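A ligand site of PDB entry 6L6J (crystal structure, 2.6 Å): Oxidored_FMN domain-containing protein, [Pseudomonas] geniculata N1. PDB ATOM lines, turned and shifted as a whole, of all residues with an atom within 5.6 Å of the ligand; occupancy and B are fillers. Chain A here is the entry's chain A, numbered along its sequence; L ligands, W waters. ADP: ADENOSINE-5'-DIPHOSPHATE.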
ATOM      1  N   ILE A 394      15.754 -27.562   0.253  1.00  0.00           N
ATOM      2  CA  ILE A 394      14.281 -27.394   0.119  1.00  0.00           C
ATOM      3  C   ILE A 394      13.851 -26.212   0.985  1.00  0.00           C
ATOM      4  O   ILE A 394      13.755 -26.384   2.225  1.00  0.00           O
ATOM      5  CB  ILE A 394      13.570 -28.716   0.466  1.00  0.00           C
ATOM      6  CG1 ILE A 394      14.379 -29.912  -0.030  1.00  0.00           C
ATOM      7  CG2 ILE A 394      12.152 -28.703  -0.085  1.00  0.00           C
ATOM      8  CD1 ILE A 394      13.640 -31.225  -0.011  1.00  0.00           C
ATOM      9  N   GLY A 395      13.646 -25.051   0.370  1.00  0.00           N
ATOM     10  CA  GLY A 395      13.280 -23.804   1.074  1.00  0.00           C
ATOM     11  C   GLY A 395      14.089 -22.610   0.581  1.00  0.00           C
ATOM     12  O   GLY A 395      15.344 -22.662   0.619  1.00  0.00           O
ATOM     13  N   GLY A 396      13.402 -21.546   0.180  1.00  0.00           N
ATOM     14  CA  GLY A 396      14.028 -20.331  -0.379  1.00  0.00           C
ATOM     15  C   GLY A 396      14.104 -19.196   0.623  1.00  0.00           C
ATOM     16  O   GLY A 396      14.330 -18.079   0.188  1.00  0.00           O
ATOM     17  N   GLY A 397      13.951 -19.499   1.910  1.00  0.00           N
ATOM     18  CA  GLY A 397      14.131 -18.510   2.998  1.00  0.00           C
ATOM     19  C   GLY A 397      15.612 -18.245   3.271  1.00  0.00           C
ATOM     20  O   GLY A 397      16.486 -18.791   2.594  1.00  0.00           O
ATOM     21  N   PRO A 398      15.950 -17.407   4.273  1.00  0.00           N
ATOM     22  CA  PRO A 398      17.340 -17.104   4.574  1.00  0.00           C
ATOM     23  C   PRO A 398      18.155 -18.327   5.010  1.00  0.00           C
ATOM     24  O   PRO A 398      19.373 -18.348   4.767  1.00  0.00           O
ATOM     25  CB  PRO A 398      17.281 -16.065   5.700  1.00  0.00           C
ATOM     26  CG  PRO A 398      15.882 -16.146   6.248  1.00  0.00           C
ATOM     27  CD  PRO A 398      15.011 -16.719   5.162  1.00  0.00           C
ATOM     28  N   ALA A 399      17.507 -19.331   5.628  1.00  0.00           N
ATOM     29  CA  ALA A 399      18.161 -20.590   6.040  1.00  0.00           C
ATOM     30  C   ALA A 399      18.660 -21.322   4.790  1.00  0.00           C
ATOM     31  O   ALA A 399      19.875 -21.435   4.633  1.00  0.00           O
ATOM     32  CB  ALA A 399      17.231 -21.469   6.857  1.00  0.00           C
ATOM     33  N   GLY A 400      17.733 -21.732   3.919  1.00  0.00           N
ATOM     34  CA  GLY A 400      18.030 -22.368   2.624  1.00  0.00           C
ATOM     35  C   GLY A 400      19.119 -21.630   1.850  1.00  0.00           C
ATOM     36  O   GLY A 400      20.145 -22.271   1.462  1.00  0.00           O
ATOM     37  N   ALA A 417      15.253 -25.515  -4.304  1.00  0.00           N
ATOM     38  CA  ALA A 417      13.843 -25.432  -4.723  1.00  0.00           C
ATOM     39  C   ALA A 417      13.047 -24.594  -3.716  1.00  0.00           C
ATOM     40  O   ALA A 417      13.341 -24.678  -2.510  1.00  0.00           O
ATOM     41  CB  ALA A 417      13.277 -26.830  -4.830  1.00  0.00           C
ATOM     42  N   ASP A 418      12.072 -23.813  -4.197  1.00  0.00           N
ATOM     43  CA  ASP A 418      11.078 -23.095  -3.363  1.00  0.00           C
ATOM     44  C   ASP A 418       9.718 -23.153  -4.056  1.00  0.00           C
ATOM     45  O   ASP A 418       9.697 -23.165  -5.298  1.00  0.00           O
ATOM     46  CB  ASP A 418      11.462 -21.631  -3.134  1.00  0.00           C
ATOM     47  CG  ASP A 418      10.554 -20.941  -2.127  1.00  0.00           C
ATOM     48  OD1 ASP A 418      10.750 -21.193  -0.921  1.00  0.00           O
ATOM     49  OD2 ASP A 418       9.610 -20.195  -2.565  1.00  0.00           O
ATOM     50  N   ALA A 419       8.632 -23.161  -3.279  1.00  0.00           N
ATOM     51  CA  ALA A 419       7.253 -23.337  -3.786  1.00  0.00           C
ATOM     52  C   ALA A 419       6.704 -22.020  -4.343  1.00  0.00           C
ATOM     53  O   ALA A 419       5.693 -22.105  -5.070  1.00  0.00           O
ATOM     54  CB  ALA A 419       6.377 -23.898  -2.676  1.00  0.00           C
ATOM     55  N   GLY A 420       7.322 -20.877  -4.026  1.00  0.00           N
ATOM     56  CA  GLY A 420       6.822 -19.531  -4.370  1.00  0.00           C
ATOM     57  C   GLY A 420       7.472 -18.962  -5.624  1.00  0.00           C
ATOM     58  O   GLY A 420       8.413 -19.557  -6.123  1.00  0.00           O
ATOM     59  N   GLY A 424      13.187 -15.783  -0.950  1.00  0.00           N
ATOM     60  CA  GLY A 424      13.202 -15.043   0.339  1.00  0.00           C
ATOM     61  C   GLY A 424      12.351 -15.666   1.426  1.00  0.00           C
ATOM     62  O   GLY A 424      12.365 -15.170   2.556  1.00  0.00           O
ATOM     63  N   GLY A 425      11.611 -16.742   1.137  1.00  0.00           N
ATOM     64  CA  GLY A 425      10.686 -17.345   2.122  1.00  0.00           C
ATOM     65  C   GLY A 425       9.953 -16.261   2.891  1.00  0.00           C
ATOM     66  O   GLY A 425       9.315 -15.417   2.248  1.00  0.00           O
ATOM     67  N   ARG A 426      10.098 -16.255   4.218  1.00  0.00           N
ATOM     68  CA  ARG A 426       9.375 -15.340   5.147  1.00  0.00           C
ATOM     69  C   ARG A 426       9.684 -13.883   4.782  1.00  0.00           C
ATOM     70  O   ARG A 426       8.813 -13.026   5.018  1.00  0.00           O
ATOM     71  CB  ARG A 426       9.758 -15.626   6.593  1.00  0.00           C
ATOM     72  CG  ARG A 426      11.226 -15.396   6.901  1.00  0.00           C
ATOM     73  CD  ARG A 426      11.577 -15.914   8.298  1.00  0.00           C
ATOM     74  NE  ARG A 426      11.034 -15.052   9.318  1.00  0.00           N
ATOM     75  CZ  ARG A 426      11.135 -15.260  10.617  1.00  0.00           C
ATOM     76  NH1 ARG A 426      11.765 -16.335  11.071  1.00  0.00           N
ATOM     77  NH2 ARG A 426      10.606 -14.392  11.462  1.00  0.00           N
ATOM     78  N   LEU A 427      10.844 -13.619   4.189  1.00  0.00           N
ATOM     79  CA  LEU A 427      11.274 -12.236   3.841  1.00  0.00           C
ATOM     80  C   LEU A 427      10.585 -11.706   2.580  1.00  0.00           C
ATOM     81  O   LEU A 427      10.559 -10.463   2.448  1.00  0.00           O
ATOM     82  CB  LEU A 427      12.791 -12.173   3.698  1.00  0.00           C
ATOM     83  CG  LEU A 427      13.547 -12.201   5.022  1.00  0.00           C
ATOM     84  CD1 LEU A 427      15.061 -12.198   4.766  1.00  0.00           C
ATOM     85  CD2 LEU A 427      13.134 -11.036   5.917  1.00  0.00           C
ATOM     86  N   SER A 462       8.452 -24.766  -7.470  1.00  0.00           N
ATOM     87  CA  SER A 462       8.716 -26.204  -7.240  1.00  0.00           C
ATOM     88  C   SER A 462       8.370 -26.588  -5.807  1.00  0.00           C
ATOM     89  O   SER A 462       9.242 -26.731  -4.957  1.00  0.00           O
ATOM     90  CB  SER A 462      10.138 -26.483  -7.616  1.00  0.00           C
ATOM     91  OG  SER A 462      10.461 -25.837  -8.846  1.00  0.00           O
ATOM     92  N   PRO A 463       7.060 -26.779  -5.493  1.00  0.00           N
ATOM     93  CA  PRO A 463       6.658 -27.454  -4.263  1.00  0.00           C
ATOM     94  C   PRO A 463       7.033 -28.931  -4.410  1.00  0.00           C
ATOM     95  O   PRO A 463       6.720 -29.494  -5.434  1.00  0.00           O
ATOM     96  CB  PRO A 463       5.135 -27.210  -4.164  1.00  0.00           C
ATOM     97  CG  PRO A 463       4.701 -26.967  -5.590  1.00  0.00           C
ATOM     98  CD  PRO A 463       5.900 -26.359  -6.302  1.00  0.00           C
ATOM     99  N   LEU A 464       7.726 -29.486  -3.420  1.00  0.00           N
ATOM    100  CA  LEU A 464       8.269 -30.873  -3.457  1.00  0.00           C
ATOM    101  C   LEU A 464       7.555 -31.747  -2.417  1.00  0.00           C
ATOM    102  O   LEU A 464       7.538 -31.375  -1.230  1.00  0.00           O
ATOM    103  CB  LEU A 464       9.779 -30.835  -3.192  1.00  0.00           C
ATOM    104  CG  LEU A 464      10.625 -30.021  -4.169  1.00  0.00           C
ATOM    105  CD1 LEU A 464      12.086 -30.012  -3.764  1.00  0.00           C
ATOM    106  CD2 LEU A 464      10.474 -30.533  -5.596  1.00  0.00           C
ATOM    107  N   GLY A 465       6.945 -32.852  -2.878  1.00  0.00           N
ATOM    108  CA  GLY A 465       6.538 -33.988  -2.035  1.00  0.00           C
ATOM    109  C   GLY A 465       7.744 -34.863  -1.743  1.00  0.00           C
ATOM    110  O   GLY A 465       8.811 -34.605  -2.373  1.00  0.00           O
ATOM    111  N   ALA A 480      14.625 -26.802   4.793  1.00  0.00           N
ATOM    112  CA  ALA A 480      14.589 -25.435   5.337  1.00  0.00           C
ATOM    113  C   ALA A 480      13.209 -24.807   5.110  1.00  0.00           C
ATOM    114  O   ALA A 480      13.148 -23.609   4.759  1.00  0.00           O
ATOM    115  CB  ALA A 480      15.688 -24.644   4.683  1.00  0.00           C
ATOM    116  N   THR A 481      12.143 -25.549   5.414  1.00  0.00           N
ATOM    117  CA  THR A 481      10.734 -25.274   5.011  1.00  0.00           C
ATOM    118  C   THR A 481      10.057 -24.233   5.923  1.00  0.00           C
ATOM    119  O   THR A 481       8.829 -24.003   5.741  1.00  0.00           O
ATOM    120  CB  THR A 481       9.971 -26.602   4.941  1.00  0.00           C
ATOM    121  OG1 THR A 481      10.118 -27.281   6.187  1.00  0.00           O
ATOM    122  CG2 THR A 481      10.501 -27.505   3.842  1.00  0.00           C
ATOM    123  N   GLY A 482      10.801 -23.569   6.796  1.00  0.00           N
ATOM    124  CA  GLY A 482      10.327 -22.399   7.548  1.00  0.00           C
ATOM    125  C   GLY A 482       9.189 -22.716   8.513  1.00  0.00           C
ATOM    126  O   GLY A 482       9.026 -23.879   8.895  1.00  0.00           O
ATOM    127  N   ALA A 483       8.416 -21.690   8.906  1.00  0.00           N
ATOM    128  CA  ALA A 483       7.350 -21.784   9.923  1.00  0.00           C
ATOM    129  C   ALA A 483       6.163 -20.904   9.542  1.00  0.00           C
ATOM    130  O   ALA A 483       6.197 -20.310   8.465  1.00  0.00           O
ATOM    131  CB  ALA A 483       7.917 -21.409  11.272  1.00  0.00           C
ATOM    132  N   GLU A 622       6.866 -25.784   9.999  1.00  0.00           N
ATOM    133  CA  GLU A 622       6.454 -26.648   8.866  1.00  0.00           C
ATOM    134  C   GLU A 622       7.505 -27.749   8.706  1.00  0.00           C
ATOM    135  O   GLU A 622       8.494 -27.512   8.031  1.00  0.00           O
ATOM    136  CB  GLU A 622       6.314 -25.828   7.592  1.00  0.00           C
ATOM    137  CG  GLU A 622       5.083 -24.931   7.589  1.00  0.00           C
ATOM    138  CD  GLU A 622       3.758 -25.673   7.479  1.00  0.00           C
ATOM    139  OE1 GLU A 622       3.768 -26.881   7.118  1.00  0.00           O
ATOM    140  OE2 GLU A 622       2.720 -25.049   7.792  1.00  0.00           O
ATOM    141  N   LEU A 625       7.318 -32.673   5.936  1.00  0.00           N
ATOM    142  CA  LEU A 625       8.128 -33.275   4.843  1.00  0.00           C
ATOM    143  C   LEU A 625       9.415 -33.847   5.449  1.00  0.00           C
ATOM    144  O   LEU A 625       9.804 -34.938   5.021  1.00  0.00           O
ATOM    145  CB  LEU A 625       8.417 -32.218   3.775  1.00  0.00           C
ATOM    146  CG  LEU A 625       9.520 -32.577   2.775  1.00  0.00           C
ATOM    147  CD1 LEU A 625       9.110 -33.735   1.864  1.00  0.00           C
ATOM    148  CD2 LEU A 625       9.892 -31.352   1.945  1.00  0.00           C
ATOM    149  N   ILE A 644      16.990 -27.406   9.130  1.00  0.00           N
ATOM    150  CA  ILE A 644      17.676 -26.160   9.604  1.00  0.00           C
ATOM    151  C   ILE A 644      16.708 -24.968   9.574  1.00  0.00           C
ATOM    152  O   ILE A 644      15.779 -24.982   8.754  1.00  0.00           O
ATOM    153  CB  ILE A 644      18.917 -25.849   8.756  1.00  0.00           C
ATOM    154  CG1 ILE A 644      18.572 -25.838   7.272  1.00  0.00           C
ATOM    155  CG2 ILE A 644      20.042 -26.809   9.070  1.00  0.00           C
ATOM    156  CD1 ILE A 644      19.487 -24.943   6.462  1.00  0.00           C
ATOM    157  N   GLY A 645      16.920 -24.003  10.459  1.00  0.00           N
ATOM    158  CA  GLY A 645      16.148 -22.755  10.511  1.00  0.00           C
ATOM    159  C   GLY A 645      14.816 -22.906  11.211  1.00  0.00           C
ATOM    160  O   GLY A 645      14.708 -23.738  12.151  1.00  0.00           O
ATOM    161  N   ASP A 646      13.819 -22.109  10.795  1.00  0.00           N
ATOM    162  CA  ASP A 646      12.517 -21.999  11.490  1.00  0.00           C
ATOM    163  C   ASP A 646      11.819 -23.360  11.474  1.00  0.00           C
ATOM    164  O   ASP A 646      11.047 -23.667  12.397  1.00  0.00           O
ATOM    165  CB  ASP A 646      11.637 -20.917  10.873  1.00  0.00           C
ATOM    166  CG  ASP A 646      12.169 -19.503  11.019  1.00  0.00           C
ATOM    167  OD1 ASP A 646      12.769 -19.181  12.061  1.00  0.00           O
ATOM    168  OD2 ASP A 646      12.000 -18.746  10.075  1.00  0.00           O
ATOM    169  N   CYS A 647      12.098 -24.175  10.459  1.00  0.00           N
ATOM    170  CA  CYS A 647      11.543 -25.541  10.303  1.00  0.00           C
ATOM    171  C   CYS A 647      12.138 -26.443  11.384  1.00  0.00           C
ATOM    172  O   CYS A 647      11.401 -27.355  11.835  1.00  0.00           O
ATOM    173  CB  CYS A 647      11.705 -26.015   8.851  1.00  0.00           C
ATOM    174  SG  CYS A 647      12.650 -27.527   8.570  1.00  0.00           S
ATOM    175  N   ALA A 656      18.367 -18.186  11.294  1.00  0.00           N
ATOM    176  CA  ALA A 656      18.183 -18.861   9.995  1.00  0.00           C
ATOM    177  C   ALA A 656      19.520 -18.840   9.248  1.00  0.00           C
ATOM    178  O   ALA A 656      19.882 -19.891   8.646  1.00  0.00           O
ATOM    179  CB  ALA A 656      17.082 -18.214   9.190  1.00  0.00           C
HETATM  180  PB  ADP L   1      13.674 -19.891   7.283  1.00  0.00           P
HETATM  181  O1B ADP L   1      14.507 -19.814   6.018  1.00  0.00           O
HETATM  182  O2B ADP L   1      13.828 -18.668   8.189  1.00  0.00           O
HETATM  183  O3B ADP L   1      13.853 -21.198   8.016  1.00  0.00           O
HETATM  184  PA  ADP L   1      11.316 -19.321   5.637  1.00  0.00           P
HETATM  185  O1A ADP L   1      11.960 -18.024   5.294  1.00  0.00           O
HETATM  186  O2A ADP L   1       9.900 -19.326   6.060  1.00  0.00           O
HETATM  187  O3A ADP L   1      12.141 -19.955   6.837  1.00  0.00           O
HETATM  188  O5' ADP L   1      11.570 -20.381   4.445  1.00  0.00           O
HETATM  189  C5' ADP L   1      10.617 -21.410   4.112  1.00  0.00           C
HETATM  190  C4' ADP L   1      10.416 -21.443   2.609  1.00  0.00           C
HETATM  191  O4' ADP L   1      10.312 -22.819   2.186  1.00  0.00           O
HETATM  192  C3' ADP L   1       9.126 -20.770   2.105  1.00  0.00           C
HETATM  193  O3' ADP L   1       9.276 -20.159   0.823  1.00  0.00           O
HETATM  194  C2' ADP L   1       8.169 -21.967   2.027  1.00  0.00           C
HETATM  195  O2' ADP L   1       6.999 -21.768   1.266  1.00  0.00           O
HETATM  196  C1' ADP L   1       9.136 -22.971   1.425  1.00  0.00           C
HETATM  197  N9  ADP L   1       8.672 -24.357   1.447  1.00  0.00           N
HETATM  198  C8  ADP L   1       7.951 -24.996   2.433  1.00  0.00           C
HETATM  199  N7  ADP L   1       7.662 -26.241   2.137  1.00  0.00           N
HETATM  200  C5  ADP L   1       8.207 -26.432   0.862  1.00  0.00           C
HETATM  201  C6  ADP L   1       8.237 -27.547  -0.005  1.00  0.00           C
HETATM  202  N6  ADP L   1       7.720 -28.724   0.275  1.00  0.00           N
HETATM  203  N1  ADP L   1       8.875 -27.400  -1.197  1.00  0.00           N
HETATM  204  C2  ADP L   1       9.422 -26.206  -1.483  1.00  0.00           C
HETATM  205  N3  ADP L   1       9.456 -25.103  -0.731  1.00  0.00           N
HETATM  206  C4  ADP L   1       8.827 -25.274   0.435  1.00  0.00           C
HETATM  207  O   HOH W   1       9.408 -18.995   8.692  1.00  0.00           O
HETATM  208  O   HOH W   2      10.564 -17.619  -1.186  1.00  0.00           O
HETATM  209  O   HOH W   3      14.801 -21.656   3.996  1.00  0.00           O
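The side-chain carboxylate (OD1) of Asp 418 is in hydrogen-bond range of an oxygen (O3') of the ligand.
O3B of the ligand sits at hydrogen-bond distance from N of Asp 646.
OD2 of Asp 646 lies close to O2B of the ligand.
The backbone NH of Arg 426 sits at hydrogen-bond distance from an oxygen (O1A) of the ligand (2.8 Å).
N of Leu 464 sits at hydrogen-bond distance from N1 of the ligand (3.3 Å).
The backbone carbonyl oxygen of Leu 464 lies within hydrogen-bond range of a nitrogen (N6) of the ligand, at 3.1 Å.
The backbone NH (N) of Ala 399 is in hydrogen-bond range of an oxygen (O1B) of the ligand (3.1 Å).
The backbone NH (N) of Ala 419 lies within hydrogen-bond range of a nitrogen (N3) of the ligand (3.3 Å).
The backbone carbonyl oxygen (O) of Asp 418 is in hydrogen-bond range of the backbone NH (N) of Ser 462, at 3.0 Å.
OD1 of Asp 418 is in hydrogen-bond range of N of Gly 396.
The side-chain carboxylate of Asp 418 is in hydrogen-bond range of the backbone NH of Gly 420, at 2.8 Å.
NH1 of Arg 426 lies within salt-bridge range of OD2 of Asp 646, 2.6 Å away.
N of Gly 395 lies within hydrogen-bond range of O of Ala 417 (2.9 Å).
The side-chain hydroxyl (OG1) of Thr 481 sits close to the side-chain sulfur (SG) of Cys 647 (3.5 Å).
The side-chain hydroxyl (OG1) of Thr 481 sits at hydrogen-bond distance from the backbone carbonyl oxygen (O) of Glu 622 (2.5 Å).
The backbone carbonyl oxygen (O) of Gly 396 lies within hydrogen-bond range of the backbone NH (N) of Gly 424.
The backbone nitrogen (N) of Pro 398 sits close to an oxygen (O1B) of the ligand, 3.3 Å away.
Merely in contact with the ligand: Gly 482 (3.1 Å), Gly 397 (3.2 Å), Gly 395 (3.3 Å), Thr 481 (3.4 Å), Gly 425 (3.4 Å), Ala 480 (3.4 Å), Ala 656 (3.4 Å), Ser 462 (3.5 Å), Ile 394 (3.7 Å), Gly 645 (3.7 Å), Pro 463 (3.8 Å), Leu 625 (3.8 Å), Gly 396 (3.9 Å), Gly 424 (3.98 Å) and Ala 483 (3.99 Å).
Hydrophobic or aromatic side chains within 4 Å of the ligand: Ile 394, Pro 398, Ala 399, Ala 419, Leu 625 and Ala 656.
Within 4 Å of the ligand: Ile 394, Gly 395, Gly 396, Gly 397, Pro 398, Ala 399, Asp 418, Ala 419, Gly 424, Gly 425, Arg 426, Ser 462, Pro 463, Leu 464, Ala 480, Thr 481, Gly 482, Ala 483, Leu 625, Gly 645, Asp 646 and Ala 656.
The nearest printed residue that does not touch the ligand is Cys 647 (4.2 Å).
Water W1 lies within hydrogen-bond range of an oxygen (O2A) of the ligand (2.7 Å), the backbone NH (N) of Ala 483 (2.9 Å) and the side-chain carboxylate (OD2) of Asp 646 (2.9 Å).
Water W3 lies within hydrogen-bond range of O of Ala 480, O1B of the ligand, N of Gly 400 and N of Gly 397.
Water W2 lies within hydrogen-bond range of N of Gly 425 (2.7 Å), OD2 of Asp 418 (3.1 Å), N of Gly 424 (3.2 Å) and O3' of the ligand (3.5 Å).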
